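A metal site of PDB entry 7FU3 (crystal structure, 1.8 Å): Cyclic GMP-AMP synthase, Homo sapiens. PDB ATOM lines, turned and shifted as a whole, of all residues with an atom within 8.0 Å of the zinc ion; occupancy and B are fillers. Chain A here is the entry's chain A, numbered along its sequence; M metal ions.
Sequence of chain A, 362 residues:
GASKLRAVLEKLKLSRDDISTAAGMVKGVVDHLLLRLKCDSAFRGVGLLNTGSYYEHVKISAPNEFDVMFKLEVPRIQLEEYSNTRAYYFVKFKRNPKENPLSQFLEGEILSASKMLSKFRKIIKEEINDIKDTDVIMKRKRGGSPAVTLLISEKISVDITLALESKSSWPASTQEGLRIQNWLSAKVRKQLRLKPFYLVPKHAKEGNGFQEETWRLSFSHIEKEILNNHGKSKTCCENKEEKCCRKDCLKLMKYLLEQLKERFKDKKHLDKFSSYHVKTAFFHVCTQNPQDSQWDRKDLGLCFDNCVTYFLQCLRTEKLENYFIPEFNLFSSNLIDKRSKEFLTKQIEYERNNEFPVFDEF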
ATOM      1  N   LEU A 227     -18.901 -27.668 -29.179  1.00  0.00           N
ATOM      2  CA  LEU A 227     -19.522 -28.969 -28.950  1.00  0.00           C
ATOM      3  C   LEU A 227     -19.099 -29.566 -27.619  1.00  0.00           C
ATOM      4  O   LEU A 227     -19.874 -30.298 -27.005  1.00  0.00           O
ATOM      5  CB  LEU A 227     -19.176 -29.957 -30.066  1.00  0.00           C
ATOM      6  CG  LEU A 227     -20.054 -29.820 -31.295  1.00  0.00           C
ATOM      7  CD1 LEU A 227     -19.445 -30.565 -32.475  1.00  0.00           C
ATOM      8  CD2 LEU A 227     -21.426 -30.375 -30.957  1.00  0.00           C
ATOM      9  N   ASN A 228     -17.866 -29.285 -27.182  1.00  0.00           N
ATOM     10  CA  ASN A 228     -17.328 -29.854 -25.962  1.00  0.00           C
ATOM     11  C   ASN A 228     -17.544 -28.984 -24.745  1.00  0.00           C
ATOM     12  O   ASN A 228     -17.121 -29.355 -23.654  1.00  0.00           O
ATOM     13  CB  ASN A 228     -15.834 -30.133 -26.131  1.00  0.00           C
ATOM     14  CG  ASN A 228     -15.547 -31.327 -27.034  1.00  0.00           C
ATOM     15  OD1 ASN A 228     -16.459 -32.094 -27.366  1.00  0.00           O
ATOM     16  ND2 ASN A 228     -14.290 -31.485 -27.433  1.00  0.00           N
ATOM     17  N   ASN A 229     -18.120 -27.808 -24.908  1.00  0.00           N
ATOM     18  CA  ASN A 229     -18.456 -26.925 -23.823  1.00  0.00           C
ATOM     19  C   ASN A 229     -19.741 -26.247 -24.298  1.00  0.00           C
ATOM     20  O   ASN A 229     -19.767 -25.097 -24.691  1.00  0.00           O
ATOM     21  CB  ASN A 229     -17.313 -25.952 -23.547  1.00  0.00           C
ATOM     22  CG  ASN A 229     -17.538 -25.112 -22.342  1.00  0.00           C
ATOM     23  OD1 ASN A 229     -18.537 -25.275 -21.630  1.00  0.00           O
ATOM     24  ND2 ASN A 229     -16.615 -24.215 -22.082  1.00  0.00           N
ATOM     25  N   HIS A 230     -20.816 -27.023 -24.298  1.00  0.00           N
ATOM     26  CA  HIS A 230     -22.010 -26.769 -25.098  1.00  0.00           C
ATOM     27  C   HIS A 230     -23.214 -26.276 -24.306  1.00  0.00           C
ATOM     28  O   HIS A 230     -24.283 -26.070 -24.903  1.00  0.00           O
ATOM     29  CB  HIS A 230     -22.404 -28.060 -25.811  1.00  0.00           C
ATOM     30  CG  HIS A 230     -22.653 -29.198 -24.859  1.00  0.00           C
ATOM     31  ND1 HIS A 230     -21.890 -30.344 -24.871  1.00  0.00           N
ATOM     32  CD2 HIS A 230     -23.547 -29.349 -23.850  1.00  0.00           C
ATOM     33  CE1 HIS A 230     -22.314 -31.156 -23.913  1.00  0.00           C
ATOM     34  NE2 HIS A 230     -23.316 -30.572 -23.282  1.00  0.00           N
ATOM     35  N   GLY A 231     -23.113 -26.124 -23.007  1.00  0.00           N
ATOM     36  CA  GLY A 231     -24.282 -25.819 -22.226  1.00  0.00           C
ATOM     37  C   GLY A 231     -24.397 -24.342 -21.925  1.00  0.00           C
ATOM     38  O   GLY A 231     -23.428 -23.604 -21.962  1.00  0.00           O
ATOM     39  N   LYS A 232     -25.620 -23.912 -21.629  1.00  0.00           N
ATOM     40  CA  LYS A 232     -25.762 -22.597 -21.012  1.00  0.00           C
ATOM     41  C   LYS A 232     -25.127 -22.610 -19.638  1.00  0.00           C
ATOM     42  O   LYS A 232     -24.423 -21.666 -19.243  1.00  0.00           O
ATOM     43  CB  LYS A 232     -27.221 -22.192 -20.883  1.00  0.00           C
ATOM     44  CG  LYS A 232     -27.287 -20.901 -20.060  1.00  0.00           C
ATOM     45  CD  LYS A 232     -28.671 -20.251 -20.024  1.00  0.00           C
ATOM     46  CE  LYS A 232     -29.102 -19.801 -21.396  1.00  0.00           C
ATOM     47  NZ  LYS A 232     -28.178 -18.755 -21.938  1.00  0.00           N
ATOM     48  N   SER A 233     -25.327 -23.697 -18.896  1.00  0.00           N
ATOM     49  CA  SER A 233     -24.668 -23.851 -17.620  1.00  0.00           C
ATOM     50  C   SER A 233     -23.229 -24.252 -17.828  1.00  0.00           C
ATOM     51  O   SER A 233     -22.930 -25.139 -18.622  1.00  0.00           O
ATOM     52  CB  SER A 233     -25.355 -24.924 -16.800  1.00  0.00           C
ATOM     53  OG  SER A 233     -24.437 -25.326 -15.805  1.00  0.00           O
ATOM     54  N   THR A 235     -21.621 -26.082 -15.989  1.00  0.00           N
ATOM     55  CA  THR A 235     -21.450 -27.452 -15.539  1.00  0.00           C
ATOM     56  C   THR A 235     -22.359 -28.432 -16.280  1.00  0.00           C
ATOM     57  O   THR A 235     -22.550 -29.563 -15.813  1.00  0.00           O
ATOM     58  CB  THR A 235     -21.674 -27.551 -14.029  1.00  0.00           C
ATOM     59  OG1 THR A 235     -22.864 -26.837 -13.693  1.00  0.00           O
ATOM     60  CG2 THR A 235     -20.528 -26.927 -13.270  1.00  0.00           C
ATOM     61  N   CYS A 236     -22.916 -28.037 -17.419  1.00  0.00           N
ATOM     62  CA  CYS A 236     -23.689 -28.973 -18.233  1.00  0.00           C
ATOM     63  C   CYS A 236     -22.879 -30.236 -18.492  1.00  0.00           C
ATOM     64  O   CYS A 236     -21.712 -30.188 -18.898  1.00  0.00           O
ATOM     65  CB  CYS A 236     -24.079 -28.312 -19.557  1.00  0.00           C
ATOM     66  SG  CYS A 236     -25.301 -29.232 -20.473  1.00  0.00           S
ATOM     67  N   CYS A 237     -23.495 -31.386 -18.197  1.00  0.00           N
ATOM     68  CA  CYS A 237     -22.944 -32.715 -18.399  1.00  0.00           C
ATOM     69  C   CYS A 237     -21.745 -33.020 -17.500  1.00  0.00           C
ATOM     70  O   CYS A 237     -21.025 -33.983 -17.772  1.00  0.00           O
ATOM     71  CB  CYS A 237     -22.569 -32.955 -19.873  1.00  0.00           C
ATOM     72  SG  CYS A 237     -24.026 -33.142 -20.992  1.00  0.00           S
ATOM     73  N   GLU A 238     -21.499 -32.243 -16.440  1.00  0.00           N
ATOM     74  CA  GLU A 238     -20.452 -32.600 -15.483  1.00  0.00           C
ATOM     75  C   GLU A 238     -21.002 -33.243 -14.225  1.00  0.00           C
ATOM     76  O   GLU A 238     -20.223 -33.580 -13.326  1.00  0.00           O
ATOM     77  CB  GLU A 238     -19.607 -31.377 -15.106  1.00  0.00           C
ATOM     78  CG  GLU A 238     -18.835 -30.777 -16.268  1.00  0.00           C
ATOM     79  CD  GLU A 238     -17.778 -29.799 -15.822  1.00  0.00           C
ATOM     80  OE1 GLU A 238     -17.754 -29.463 -14.614  1.00  0.00           O
ATOM     81  OE2 GLU A 238     -16.961 -29.365 -16.655  1.00  0.00           O
ATOM     82  N   GLU A 242     -27.317 -32.575 -14.564  1.00  0.00           N
ATOM     83  CA  GLU A 242     -27.261 -31.733 -15.743  1.00  0.00           C
ATOM     84  C   GLU A 242     -26.773 -32.538 -16.958  1.00  0.00           C
ATOM     85  O   GLU A 242     -25.830 -32.142 -17.631  1.00  0.00           O
ATOM     86  CB  GLU A 242     -26.353 -30.540 -15.530  1.00  0.00           C
ATOM     87  CG  GLU A 242     -26.627 -29.638 -14.304  1.00  0.00           C
ATOM     88  CD  GLU A 242     -25.757 -28.409 -14.333  1.00  0.00           C
ATOM     89  OE1 GLU A 242     -25.842 -27.653 -15.333  1.00  0.00           O
ATOM     90  OE2 GLU A 242     -24.979 -28.186 -13.357  1.00  0.00           O
ATOM     91  N   LYS A 243     -27.439 -33.640 -17.261  1.00  0.00           N
ATOM     92  CA  LYS A 243     -27.126 -34.443 -18.444  1.00  0.00           C
ATOM     93  C   LYS A 243     -28.075 -34.001 -19.551  1.00  0.00           C
ATOM     94  O   LYS A 243     -29.287 -34.243 -19.475  1.00  0.00           O
ATOM     95  CB  LYS A 243     -27.290 -35.938 -18.189  1.00  0.00           C
ATOM     96  CG  LYS A 243     -26.512 -36.545 -16.990  1.00  0.00           C
ATOM     97  CD  LYS A 243     -24.991 -36.273 -17.019  1.00  0.00           C
ATOM     98  CE  LYS A 243     -24.218 -37.173 -17.952  1.00  0.00           C
ATOM     99  NZ  LYS A 243     -22.860 -36.596 -18.259  1.00  0.00           N
ATOM    100  N   CYS A 244     -27.554 -33.321 -20.559  1.00  0.00           N
ATOM    101  CA  CYS A 244     -28.347 -32.941 -21.720  1.00  0.00           C
ATOM    102  C   CYS A 244     -28.112 -33.941 -22.846  1.00  0.00           C
ATOM    103  O   CYS A 244     -27.201 -34.765 -22.783  1.00  0.00           O
ATOM    104  CB  CYS A 244     -28.000 -31.526 -22.166  1.00  0.00           C
ATOM    105  SG  CYS A 244     -26.470 -31.341 -23.102  1.00  0.00           S
ATOM    106  N   CYS A 245     -28.943 -33.879 -23.886  1.00  0.00           N
ATOM    107  CA  CYS A 245     -28.844 -34.780 -25.026  1.00  0.00           C
ATOM    108  C   CYS A 245     -28.381 -34.072 -26.302  1.00  0.00           C
ATOM    109  O   CYS A 245     -28.682 -34.516 -27.407  1.00  0.00           O
ATOM    110  CB  CYS A 245     -30.181 -35.497 -25.267  1.00  0.00           C
ATOM    111  SG  CYS A 245     -31.558 -34.361 -25.675  1.00  0.00           S
ATOM    112  N   ARG A 246     -27.681 -32.953 -26.154  1.00  0.00           N
ATOM    113  CA  ARG A 246     -27.180 -32.222 -27.321  1.00  0.00           C
ATOM    114  C   ARG A 246     -26.282 -33.120 -28.188  1.00  0.00           C
ATOM    115  O   ARG A 246     -26.526 -33.280 -29.383  1.00  0.00           O
ATOM    116  CB  ARG A 246     -26.431 -30.952 -26.885  1.00  0.00           C
ATOM    117  CG  ARG A 246     -27.331 -29.747 -26.497  1.00  0.00           C
ATOM    118  CD  ARG A 246     -26.491 -28.510 -26.292  1.00  0.00           C
ATOM    119  NE  ARG A 246     -27.185 -27.305 -25.828  1.00  0.00           N
ATOM    120  CZ  ARG A 246     -27.497 -27.077 -24.559  1.00  0.00           C
ATOM    121  NH1 ARG A 246     -28.103 -25.953 -24.245  1.00  0.00           N
ATOM    122  NH2 ARG A 246     -27.228 -27.992 -23.619  1.00  0.00           N
ATOM    123  N   LYS A 247     -25.250 -33.722 -27.592  1.00  0.00           N
ATOM    124  CA  LYS A 247     -24.340 -34.512 -28.425  1.00  0.00           C
ATOM    125  C   LYS A 247     -25.024 -35.734 -29.003  1.00  0.00           C
ATOM    126  O   LYS A 247     -24.708 -36.159 -30.117  1.00  0.00           O
ATOM    127  CB  LYS A 247     -23.100 -34.944 -27.629  1.00  0.00           C
ATOM    128  CG  LYS A 247     -22.099 -33.795 -27.341  1.00  0.00           C
ATOM    129  CD  LYS A 247     -20.814 -34.382 -26.764  1.00  0.00           C
ATOM    130  CE  LYS A 247     -19.720 -33.315 -26.617  1.00  0.00           C
ATOM    131  NZ  LYS A 247     -18.395 -33.877 -26.229  1.00  0.00           N
ATOM    132  N   ASP A 292     -30.495 -25.198 -21.253  1.00  0.00           N
ATOM    133  CA  ASP A 292     -30.233 -26.614 -21.069  1.00  0.00           C
ATOM    134  C   ASP A 292     -31.509 -27.380 -20.794  1.00  0.00           C
ATOM    135  O   ASP A 292     -31.579 -28.575 -21.082  1.00  0.00           O
ATOM    136  CB  ASP A 292     -29.230 -26.867 -19.945  1.00  0.00           C
ATOM    137  CG  ASP A 292     -27.907 -26.169 -20.163  1.00  0.00           C
ATOM    138  OD1 ASP A 292     -27.587 -25.882 -21.333  1.00  0.00           O
ATOM    139  OD2 ASP A 292     -27.212 -25.887 -19.175  1.00  0.00           O
ATOM    140  N   TRP A 295     -32.919 -29.381 -23.589  1.00  0.00           N
ATOM    141  CA  TRP A 295     -32.144 -30.532 -24.014  1.00  0.00           C
ATOM    142  C   TRP A 295     -31.994 -31.522 -22.891  1.00  0.00           C
ATOM    143  O   TRP A 295     -30.957 -32.175 -22.778  1.00  0.00           O
ATOM    144  CB  TRP A 295     -30.768 -30.112 -24.495  1.00  0.00           C
ATOM    145  CG  TRP A 295     -30.832 -29.135 -25.602  1.00  0.00           C
ATOM    146  CD1 TRP A 295     -30.859 -27.770 -25.499  1.00  0.00           C
ATOM    147  CD2 TRP A 295     -30.795 -29.435 -26.995  1.00  0.00           C
ATOM    148  NE1 TRP A 295     -30.865 -27.207 -26.761  1.00  0.00           N
ATOM    149  CE2 TRP A 295     -30.836 -28.203 -27.687  1.00  0.00           C
ATOM    150  CE3 TRP A 295     -30.770 -30.626 -27.730  1.00  0.00           C
ATOM    151  CZ2 TRP A 295     -30.835 -28.135 -29.084  1.00  0.00           C
ATOM    152  CZ3 TRP A 295     -30.775 -30.552 -29.112  1.00  0.00           C
ATOM    153  CH2 TRP A 295     -30.808 -29.323 -29.786  1.00  0.00           C
HETATM  154 ZN    ZN M   1     -24.651 -31.051 -21.761  1.00  0.00          ZN
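Of the 19 residues printed, 4 come within 4 Å of the zinc ion.
NE2 of His 230 is bound to the zinc ion (2.1 Å).
The side-chain sulfur (SG) of Cys 244 is bound to the zinc ion, at 2.3 Å.
The zinc ion is bound by SG of Cys 237, 2.3 Å away.
SG of Cys 236 binds the zinc ion.
The backbone carbonyl oxygen (O) of His 230 is in hydrogen-bond range of the guanidinium group (NE) of Arg 246 (3.3 Å).
ND1 of His 230 lies within hydrogen-bond range of O of Leu 227.
O of Cys 237 lies within hydrogen-bond range of NZ of Lys 243, at 3.2 Å.
O of Glu 242 is in hydrogen-bond range of N of Cys 237, at 2.5 Å.
SG of Cys 244 sits close to NH2 of Arg 246, at 3.5 Å.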
